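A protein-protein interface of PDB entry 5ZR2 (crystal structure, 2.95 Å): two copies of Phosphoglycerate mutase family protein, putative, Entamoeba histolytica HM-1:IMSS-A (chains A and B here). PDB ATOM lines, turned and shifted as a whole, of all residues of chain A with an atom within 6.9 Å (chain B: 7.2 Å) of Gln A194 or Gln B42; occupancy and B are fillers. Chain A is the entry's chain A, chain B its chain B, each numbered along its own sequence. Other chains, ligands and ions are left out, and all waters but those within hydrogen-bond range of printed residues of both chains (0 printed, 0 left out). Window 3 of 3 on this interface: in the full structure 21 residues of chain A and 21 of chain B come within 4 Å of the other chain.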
ATOM      1  N   GLU A  38      20.412 -15.539  -9.933  1.00  0.00           N
ATOM      2  CA  GLU A  38      20.057 -15.881 -11.301  1.00  0.00           C
ATOM      3  C   GLU A  38      18.589 -15.597 -11.615  1.00  0.00           C
ATOM      4  O   GLU A  38      18.281 -15.083 -12.687  1.00  0.00           O
ATOM      5  CB  GLU A  38      20.402 -17.338 -11.575  1.00  0.00           C
ATOM      6  CG  GLU A  38      21.900 -17.570 -11.653  1.00  0.00           C
ATOM      7  CD  GLU A  38      22.272 -19.034 -11.686  1.00  0.00           C
ATOM      8  OE1 GLU A  38      21.912 -19.711 -12.670  1.00  0.00           O
ATOM      9  OE2 GLU A  38      22.936 -19.502 -10.741  1.00  0.00           O
ATOM     10  N   GLN A  42      16.905 -12.805 -14.161  1.00  0.00           N
ATOM     11  CA  GLN A  42      15.868 -13.151 -15.140  1.00  0.00           C
ATOM     12  C   GLN A  42      14.725 -12.149 -15.109  1.00  0.00           C
ATOM     13  O   GLN A  42      14.313 -11.636 -16.146  1.00  0.00           O
ATOM     14  CB  GLN A  42      15.313 -14.547 -14.864  1.00  0.00           C
ATOM     15  CG  GLN A  42      14.068 -14.912 -15.672  1.00  0.00           C
ATOM     16  CD  GLN A  42      14.360 -15.217 -17.132  1.00  0.00           C
ATOM     17  OE1 GLN A  42      15.345 -15.885 -17.455  1.00  0.00           O
ATOM     18  NE2 GLN A  42      13.495 -14.738 -18.028  1.00  0.00           N
ATOM     19  N   ASN A 191       6.547 -23.450 -12.792  1.00  0.00           N
ATOM     20  CA  ASN A 191       7.898 -23.933 -12.497  1.00  0.00           C
ATOM     21  C   ASN A 191       8.925 -23.722 -13.605  1.00  0.00           C
ATOM     22  O   ASN A 191       9.731 -24.607 -13.913  1.00  0.00           O
ATOM     23  CB  ASN A 191       7.871 -25.405 -12.082  1.00  0.00           C
ATOM     24  CG  ASN A 191       9.199 -25.865 -11.490  1.00  0.00           C
ATOM     25  OD1 ASN A 191       9.924 -25.078 -10.873  1.00  0.00           O
ATOM     26  ND2 ASN A 191       9.523 -27.136 -11.668  1.00  0.00           N
ATOM     27  N   SER A 192       8.886 -22.538 -14.193  1.00  0.00           N
ATOM     28  CA  SER A 192       9.882 -22.136 -15.163  1.00  0.00           C
ATOM     29  C   SER A 192      11.221 -21.942 -14.432  1.00  0.00           C
ATOM     30  O   SER A 192      11.320 -21.132 -13.510  1.00  0.00           O
ATOM     31  CB  SER A 192       9.432 -20.864 -15.873  1.00  0.00           C
ATOM     32  OG  SER A 192      10.512 -20.256 -16.545  1.00  0.00           O
ATOM     33  N   THR A 193      12.224 -22.721 -14.840  1.00  0.00           N
ATOM     34  CA  THR A 193      13.553 -22.760 -14.202  1.00  0.00           C
ATOM     35  C   THR A 193      14.727 -22.586 -15.194  1.00  0.00           C
ATOM     36  O   THR A 193      15.876 -22.878 -14.850  1.00  0.00           O
ATOM     37  CB  THR A 193      13.756 -24.098 -13.445  1.00  0.00           C
ATOM     38  OG1 THR A 193      13.388 -25.189 -14.299  1.00  0.00           O
ATOM     39  CG2 THR A 193      12.920 -24.152 -12.183  1.00  0.00           C
ATOM     40  N   GLN A 194      14.449 -22.088 -16.402  1.00  0.00           N
ATOM     41  CA  GLN A 194      15.481 -21.920 -17.458  1.00  0.00           C
ATOM     42  C   GLN A 194      16.643 -20.989 -17.105  1.00  0.00           C
ATOM     43  O   GLN A 194      17.711 -21.080 -17.707  1.00  0.00           O
ATOM     44  CB  GLN A 194      14.845 -21.439 -18.760  1.00  0.00           C
ATOM     45  CG  GLN A 194      14.011 -22.504 -19.437  1.00  0.00           C
ATOM     46  CD  GLN A 194      13.309 -22.027 -20.704  1.00  0.00           C
ATOM     47  OE1 GLN A 194      12.946 -20.859 -20.856  1.00  0.00           O
ATOM     48  NE2 GLN A 194      13.087 -22.955 -21.608  1.00  0.00           N
ATOM     49  N   HIS A 195      16.412 -20.095 -16.147  1.00  0.00           N
ATOM     50  CA  HIS A 195      17.446 -19.203 -15.585  1.00  0.00           C
ATOM     51  C   HIS A 195      18.571 -19.880 -14.766  1.00  0.00           C
ATOM     52  O   HIS A 195      19.571 -19.230 -14.452  1.00  0.00           O
ATOM     53  CB  HIS A 195      16.789 -18.108 -14.729  1.00  0.00           C
ATOM     54  CG  HIS A 195      16.012 -18.634 -13.559  1.00  0.00           C
ATOM     55  ND1 HIS A 195      14.684 -18.986 -13.650  1.00  0.00           N
ATOM     56  CD2 HIS A 195      16.376 -18.873 -12.277  1.00  0.00           C
ATOM     57  CE1 HIS A 195      14.266 -19.426 -12.479  1.00  0.00           C
ATOM     58  NE2 HIS A 195      15.272 -19.366 -11.627  1.00  0.00           N
ATOM     59  N   LEU A 196      18.408 -21.159 -14.421  1.00  0.00           N
ATOM     60  CA  LEU A 196      19.416 -21.918 -13.664  1.00  0.00           C
ATOM     61  C   LEU A 196      20.362 -22.704 -14.571  1.00  0.00           C
ATOM     62  O   LEU A 196      19.968 -23.154 -15.649  1.00  0.00           O
ATOM     63  CB  LEU A 196      18.737 -22.881 -12.682  1.00  0.00           C
ATOM     64  CG  LEU A 196      17.785 -22.292 -11.632  1.00  0.00           C
ATOM     65  CD1 LEU A 196      17.360 -23.384 -10.664  1.00  0.00           C
ATOM     66  CD2 LEU A 196      18.405 -21.129 -10.866  1.00  0.00           C
ATOM     67  N   LEU A 197      21.609 -22.859 -14.115  1.00  0.00           N
ATOM     68  CA  LEU A 197      22.669 -23.545 -14.862  1.00  0.00           C
ATOM     69  C   LEU A 197      23.117 -24.776 -14.067  1.00  0.00           C
ATOM     70  O   LEU A 197      23.627 -25.754 -14.622  1.00  0.00           O
ATOM     71  CB  LEU A 197      23.863 -22.603 -15.080  1.00  0.00           C
ATOM     72  CG  LEU A 197      23.771 -21.313 -15.936  1.00  0.00           C
ATOM     73  CD1 LEU A 197      22.367 -20.904 -16.376  1.00  0.00           C
ATOM     74  CD2 LEU A 197      24.424 -20.151 -15.189  1.00  0.00           C
ATOM     75  N   ALA B  36      11.767 -20.363 -32.957  1.00  0.00           N
ATOM     76  CA  ALA B  36      12.207 -21.748 -33.171  1.00  0.00           C
ATOM     77  C   ALA B  36      13.711 -21.923 -32.954  1.00  0.00           C
ATOM     78  O   ALA B  36      14.149 -22.906 -32.353  1.00  0.00           O
ATOM     79  CB  ALA B  36      11.813 -22.222 -34.562  1.00  0.00           C
ATOM     80  N   ASN B  37      14.488 -20.962 -33.448  1.00  0.00           N
ATOM     81  CA  ASN B  37      15.932 -20.918 -33.208  1.00  0.00           C
ATOM     82  C   ASN B  37      16.210 -20.855 -31.718  1.00  0.00           C
ATOM     83  O   ASN B  37      16.973 -21.658 -31.183  1.00  0.00           O
ATOM     84  CB  ASN B  37      16.576 -19.680 -33.848  1.00  0.00           C
ATOM     85  CG  ASN B  37      16.417 -19.632 -35.356  1.00  0.00           C
ATOM     86  OD1 ASN B  37      16.431 -20.663 -36.029  1.00  0.00           O
ATOM     87  ND2 ASN B  37      16.273 -18.422 -35.898  1.00  0.00           N
ATOM     88  N   GLU B  38      15.572 -19.889 -31.066  1.00  0.00           N
ATOM     89  CA  GLU B  38      15.775 -19.620 -29.648  1.00  0.00           C
ATOM     90  C   GLU B  38      15.462 -20.829 -28.761  1.00  0.00           C
ATOM     91  O   GLU B  38      16.252 -21.151 -27.879  1.00  0.00           O
ATOM     92  CB  GLU B  38      14.957 -18.395 -29.229  1.00  0.00           C
ATOM     93  CG  GLU B  38      15.570 -17.086 -29.708  1.00  0.00           C
ATOM     94  CD  GLU B  38      14.591 -15.925 -29.726  1.00  0.00           C
ATOM     95  OE1 GLU B  38      13.710 -15.863 -28.849  1.00  0.00           O
ATOM     96  OE2 GLU B  38      14.705 -15.064 -30.623  1.00  0.00           O
ATOM     97  N   VAL B  39      14.336 -21.501 -29.007  1.00  0.00           N
ATOM     98  CA  VAL B  39      13.985 -22.711 -28.243  1.00  0.00           C
ATOM     99  C   VAL B  39      14.976 -23.852 -28.533  1.00  0.00           C
ATOM    100  O   VAL B  39      15.368 -24.577 -27.618  1.00  0.00           O
ATOM    101  CB  VAL B  39      12.499 -23.137 -28.428  1.00  0.00           C
ATOM    102  CG1 VAL B  39      12.240 -23.807 -29.771  1.00  0.00           C
ATOM    103  CG2 VAL B  39      12.051 -24.051 -27.293  1.00  0.00           C
ATOM    104  N   ALA B  40      15.392 -23.982 -29.794  1.00  0.00           N
ATOM    105  CA  ALA B  40      16.429 -24.944 -30.191  1.00  0.00           C
ATOM    106  C   ALA B  40      17.743 -24.702 -29.445  1.00  0.00           C
ATOM    107  O   ALA B  40      18.357 -25.645 -28.935  1.00  0.00           O
ATOM    108  CB  ALA B  40      16.666 -24.870 -31.689  1.00  0.00           C
ATOM    109  N   GLN B  41      18.159 -23.435 -29.407  1.00  0.00           N
ATOM    110  CA  GLN B  41      19.330 -22.976 -28.633  1.00  0.00           C
ATOM    111  C   GLN B  41      19.244 -23.290 -27.141  1.00  0.00           C
ATOM    112  O   GLN B  41      20.265 -23.560 -26.525  1.00  0.00           O
ATOM    113  CB  GLN B  41      19.512 -21.458 -28.756  1.00  0.00           C
ATOM    114  CG  GLN B  41      19.975 -20.930 -30.106  1.00  0.00           C
ATOM    115  CD  GLN B  41      19.731 -19.422 -30.262  1.00  0.00           C
ATOM    116  OE1 GLN B  41      19.611 -18.688 -29.273  1.00  0.00           O
ATOM    117  NE2 GLN B  41      19.660 -18.955 -31.510  1.00  0.00           N
ATOM    118  N   GLN B  42      18.046 -23.183 -26.563  1.00  0.00           N
ATOM    119  CA  GLN B  42      17.814 -23.514 -25.149  1.00  0.00           C
ATOM    120  C   GLN B  42      17.973 -25.012 -24.912  1.00  0.00           C
ATOM    121  O   GLN B  42      18.735 -25.430 -24.035  1.00  0.00           O
ATOM    122  CB  GLN B  42      16.413 -23.069 -24.709  1.00  0.00           C
ATOM    123  CG  GLN B  42      15.984 -23.519 -23.310  1.00  0.00           C
ATOM    124  CD  GLN B  42      16.535 -22.641 -22.199  1.00  0.00           C
ATOM    125  OE1 GLN B  42      16.436 -21.412 -22.262  1.00  0.00           O
ATOM    126  NE2 GLN B  42      17.099 -23.265 -21.162  1.00  0.00           N
ATOM    127  N   ILE B  43      17.229 -25.801 -25.688  1.00  0.00           N
ATOM    128  CA  ILE B  43      17.237 -27.269 -25.574  1.00  0.00           C
ATOM    129  C   ILE B  43      18.655 -27.835 -25.747  1.00  0.00           C
ATOM    130  O   ILE B  43      19.001 -28.799 -25.079  1.00  0.00           O
ATOM    131  CB  ILE B  43      16.257 -27.936 -26.581  1.00  0.00           C
ATOM    132  CG1 ILE B  43      14.789 -27.564 -26.278  1.00  0.00           C
ATOM    133  CG2 ILE B  43      16.412 -29.457 -26.607  1.00  0.00           C
ATOM    134  CD1 ILE B  43      14.158 -28.227 -25.068  1.00  0.00           C
ATOM    135  N   LYS B  44      19.457 -27.235 -26.632  1.00  0.00           N
ATOM    136  CA  LYS B  44      20.868 -27.629 -26.863  1.00  0.00           C
ATOM    137  C   LYS B  44      21.046 -29.108 -27.216  1.00  0.00           C
ATOM    138  O   LYS B  44      21.980 -29.755 -26.747  1.00  0.00           O
ATOM    139  CB  LYS B  44      21.752 -27.281 -25.648  1.00  0.00           C
ATOM    140  CG  LYS B  44      22.086 -25.811 -25.517  1.00  0.00           C
ATOM    141  CD  LYS B  44      23.013 -25.526 -24.339  1.00  0.00           C
ATOM    142  CE  LYS B  44      22.287 -25.521 -22.998  1.00  0.00           C
ATOM    143  NZ  LYS B  44      21.347 -24.370 -22.835  1.00  0.00           N
ATOM    144  N   GLY B  45      20.145 -29.653 -28.028  1.00  0.00           N
ATOM    145  CA  GLY B  45      20.215 -31.076 -28.393  1.00  0.00           C
ATOM    146  C   GLY B  45      20.119 -32.065 -27.233  1.00  0.00           C
ATOM    147  O   GLY B  45      20.486 -33.228 -27.383  1.00  0.00           O
ATOM    148  N   ASN B  46      19.588 -31.604 -26.097  1.00  0.00           N
ATOM    149  CA  ASN B  46      19.620 -32.322 -24.815  1.00  0.00           C
ATOM    150  C   ASN B  46      18.385 -33.223 -24.642  1.00  0.00           C
ATOM    151  O   ASN B  46      17.555 -33.037 -23.753  1.00  0.00           O
ATOM    152  CB  ASN B  46      19.739 -31.295 -23.678  1.00  0.00           C
ATOM    153  CG  ASN B  46      19.916 -31.922 -22.308  1.00  0.00           C
ATOM    154  OD1 ASN B  46      20.166 -33.126 -22.172  1.00  0.00           O
ATOM    155  ND2 ASN B  46      19.769 -31.097 -21.272  1.00  0.00           N
ATOM    156  N   THR B 173       6.436 -21.822 -28.929  1.00  0.00           N
ATOM    157  CA  THR B 173       7.652 -22.428 -28.354  1.00  0.00           C
ATOM    158  C   THR B 173       7.626 -22.502 -26.818  1.00  0.00           C
ATOM    159  O   THR B 173       8.665 -22.433 -26.175  1.00  0.00           O
ATOM    160  CB  THR B 173       8.960 -21.762 -28.854  1.00  0.00           C
ATOM    161  OG1 THR B 173       9.102 -20.448 -28.302  1.00  0.00           O
ATOM    162  CG2 THR B 173       8.993 -21.701 -30.375  1.00  0.00           C
ATOM    163  N   GLY B 174       6.434 -22.669 -26.249  1.00  0.00           N
ATOM    164  CA  GLY B 174       6.265 -22.819 -24.811  1.00  0.00           C
ATOM    165  C   GLY B 174       6.608 -24.239 -24.420  1.00  0.00           C
ATOM    166  O   GLY B 174       6.033 -25.184 -24.963  1.00  0.00           O
ATOM    167  N   ILE B 175       7.554 -24.389 -23.495  1.00  0.00           N
ATOM    168  CA  ILE B 175       7.999 -25.707 -23.047  1.00  0.00           C
ATOM    169  C   ILE B 175       7.124 -26.171 -21.883  1.00  0.00           C
ATOM    170  O   ILE B 175       6.781 -25.393 -20.991  1.00  0.00           O
ATOM    171  CB  ILE B 175       9.501 -25.727 -22.662  1.00  0.00           C
ATOM    172  CG1 ILE B 175      10.343 -25.298 -23.871  1.00  0.00           C
ATOM    173  CG2 ILE B 175       9.920 -27.122 -22.178  1.00  0.00           C
ATOM    174  CD1 ILE B 175      11.840 -25.330 -23.659  1.00  0.00           C
ATOM    175  N   SER B 192       6.993 -22.786 -20.208  1.00  0.00           N
ATOM    176  CA  SER B 192       8.243 -22.088 -19.938  1.00  0.00           C
ATOM    177  C   SER B 192       8.714 -21.416 -21.225  1.00  0.00           C
ATOM    178  O   SER B 192       8.939 -22.092 -22.225  1.00  0.00           O
ATOM    179  CB  SER B 192       9.298 -23.063 -19.419  1.00  0.00           C
ATOM    180  OG  SER B 192      10.554 -22.424 -19.255  1.00  0.00           O
ATOM    181  N   THR B 193       8.836 -20.088 -21.183  1.00  0.00           N
ATOM    182  CA  THR B 193       9.187 -19.257 -22.349  1.00  0.00           C
ATOM    183  C   THR B 193      10.263 -18.194 -22.035  1.00  0.00           C
ATOM    184  O   THR B 193      10.252 -17.103 -22.611  1.00  0.00           O
ATOM    185  CB  THR B 193       7.937 -18.533 -22.894  1.00  0.00           C
ATOM    186  OG1 THR B 193       7.292 -17.830 -21.825  1.00  0.00           O
ATOM    187  CG2 THR B 193       6.960 -19.510 -23.510  1.00  0.00           C
ATOM    188  N   GLN B 194      11.198 -18.517 -21.138  1.00  0.00           N
ATOM    189  CA  GLN B 194      12.303 -17.597 -20.790  1.00  0.00           C
ATOM    190  C   GLN B 194      13.372 -17.485 -21.881  1.00  0.00           C
ATOM    191  O   GLN B 194      14.160 -16.544 -21.877  1.00  0.00           O
ATOM    192  CB  GLN B 194      12.964 -17.994 -19.468  1.00  0.00           C
ATOM    193  CG  GLN B 194      12.002 -18.064 -18.295  1.00  0.00           C
ATOM    194  CD  GLN B 194      12.701 -18.332 -16.966  1.00  0.00           C
ATOM    195  OE1 GLN B 194      13.557 -19.212 -16.860  1.00  0.00           O
ATOM    196  NE2 GLN B 194      12.315 -17.591 -15.940  1.00  0.00           N
ATOM    197  N   HIS B 195      13.395 -18.450 -22.799  1.00  0.00           N
ATOM    198  CA  HIS B 195      14.278 -18.420 -23.987  1.00  0.00           C
ATOM    199  C   HIS B 195      13.961 -17.333 -25.022  1.00  0.00           C
ATOM    200  O   HIS B 195      14.788 -17.060 -25.894  1.00  0.00           O
ATOM    201  CB  HIS B 195      14.309 -19.787 -24.702  1.00  0.00           C
ATOM    202  CG  HIS B 195      12.959 -20.309 -25.094  1.00  0.00           C
ATOM    203  ND1 HIS B 195      12.254 -21.179 -24.298  1.00  0.00           N
ATOM    204  CD2 HIS B 195      12.188 -20.092 -26.185  1.00  0.00           C
ATOM    205  CE1 HIS B 195      11.105 -21.474 -24.872  1.00  0.00           C
ATOM    206  NE2 HIS B 195      11.038 -20.827 -26.021  1.00  0.00           N
ATOM    207  N   LEU B 196      12.777 -16.732 -24.934  1.00  0.00           N
ATOM    208  CA  LEU B 196      12.337 -15.705 -25.883  1.00  0.00           C
ATOM    209  C   LEU B 196      12.803 -14.290 -25.522  1.00  0.00           C
ATOM    210  O   LEU B 196      12.613 -13.838 -24.395  1.00  0.00           O
ATOM    211  CB  LEU B 196      10.810 -15.749 -26.027  1.00  0.00           C
ATOM    212  CG  LEU B 196      10.265 -17.074 -26.581  1.00  0.00           C
ATOM    213  CD1 LEU B 196       8.748 -17.059 -26.634  1.00  0.00           C
ATOM    214  CD2 LEU B 196      10.832 -17.377 -27.962  1.00  0.00           C
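Gln A42 touches Gln B194. OE1 of Gln B194 touches C of Thr A193, at 3.9 Å. Gln A194 touches Gln B42 (NE2 to CG, 3.4 Å). Gln A194 touches Ile B175. Gln A194 touches Thr B193.
The backbone carbonyl oxygen of Gln B42 is in hydrogen-bond range of the side-chain amino group of Lys B44 (3.1 Å). A ring nitrogen (NE2) of His B195 lies within hydrogen-bond range of the backbone carbonyl oxygen (O) of Thr B173. The backbone carbonyl oxygen (O) of Ile B175 sits at hydrogen-bond distance from the backbone NH (N) of Ser B192 (2.7 Å).
Hydrophobic or aromatic side chains of chain B within 4 Å of the printed part of chain A: Ile B175 and His B195. Along chain B the printed residues that touch a printed residue of chain A span positions 42 to 195. Hydrophobic or aromatic side chains of chain A within 4 Å of the printed part of chain B: His A195.
Gln A42 touches Gln B194, and with the chains exchanged Gln A194 touches Gln B42. Ser A192 touches its own counterpart, Ser B192. Ser A192 touches Gln B194, and with the chains exchanged Gln A194 touches Ser B192. Gln B194 touches its own counterpart, Gln A194. 7 positions are printed for both chains. Of the 11 pairs that touch across the chains among the printed residues, 10 have their exchanged pair printed and touching as well.
Of the printed residues of chain B, Thr A193 touches Gln B194. Gln A194 touches just these residues of chain B: Gln B42 (3.4 Å), Ile B175 (3.4 Å), Ser B192 (3.1 Å), Thr B193 (3.96 Å), Gln B194 (2.9 Å) and His B195 (3.1 Å). Of the printed residues of chain B, His A195 touches Gln B194. Gln B42 touches just one residue of chain A: Gln A194 (3.4 Å). Of the printed residues of chain A, Ile B175 touches Gln A194 (3.4 Å). Printed residues of chain A within 4 Å of Thr B193: Gln A194. Printed residues of chain A within 4 Å of His B195: Gln A194 (3.1 Å). The nearest residue of chain B that does not touch Gln A194 is Leu B196 (5.8 Å). The nearest residue of chain A that does not touch Gln B42 is His A195 (6.0 Å).
OG of Ser B192 lies within hydrogen-bond range of OG of Ser A192 (3.5 Å). OE1 of Gln B194 lies close to OG of Ser A192, 3.2 Å away. The side-chain amide oxygen (OE1) of Gln A194 lies close to the side-chain hydroxyl (OG) of Ser B192, 3.3 Å away. The side-chain amide oxygen (OE1) of Gln A194 is in hydrogen-bond range of the backbone NH (N) of Gln B194, at 2.9 Å. The side-chain amide oxygen of Gln A194 sits at hydrogen-bond distance from the backbone NH of His B195 (3.1 Å). The side-chain amide oxygen (OE1) of Gln B194 is in hydrogen-bond range of the backbone NH (N) of His A195.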
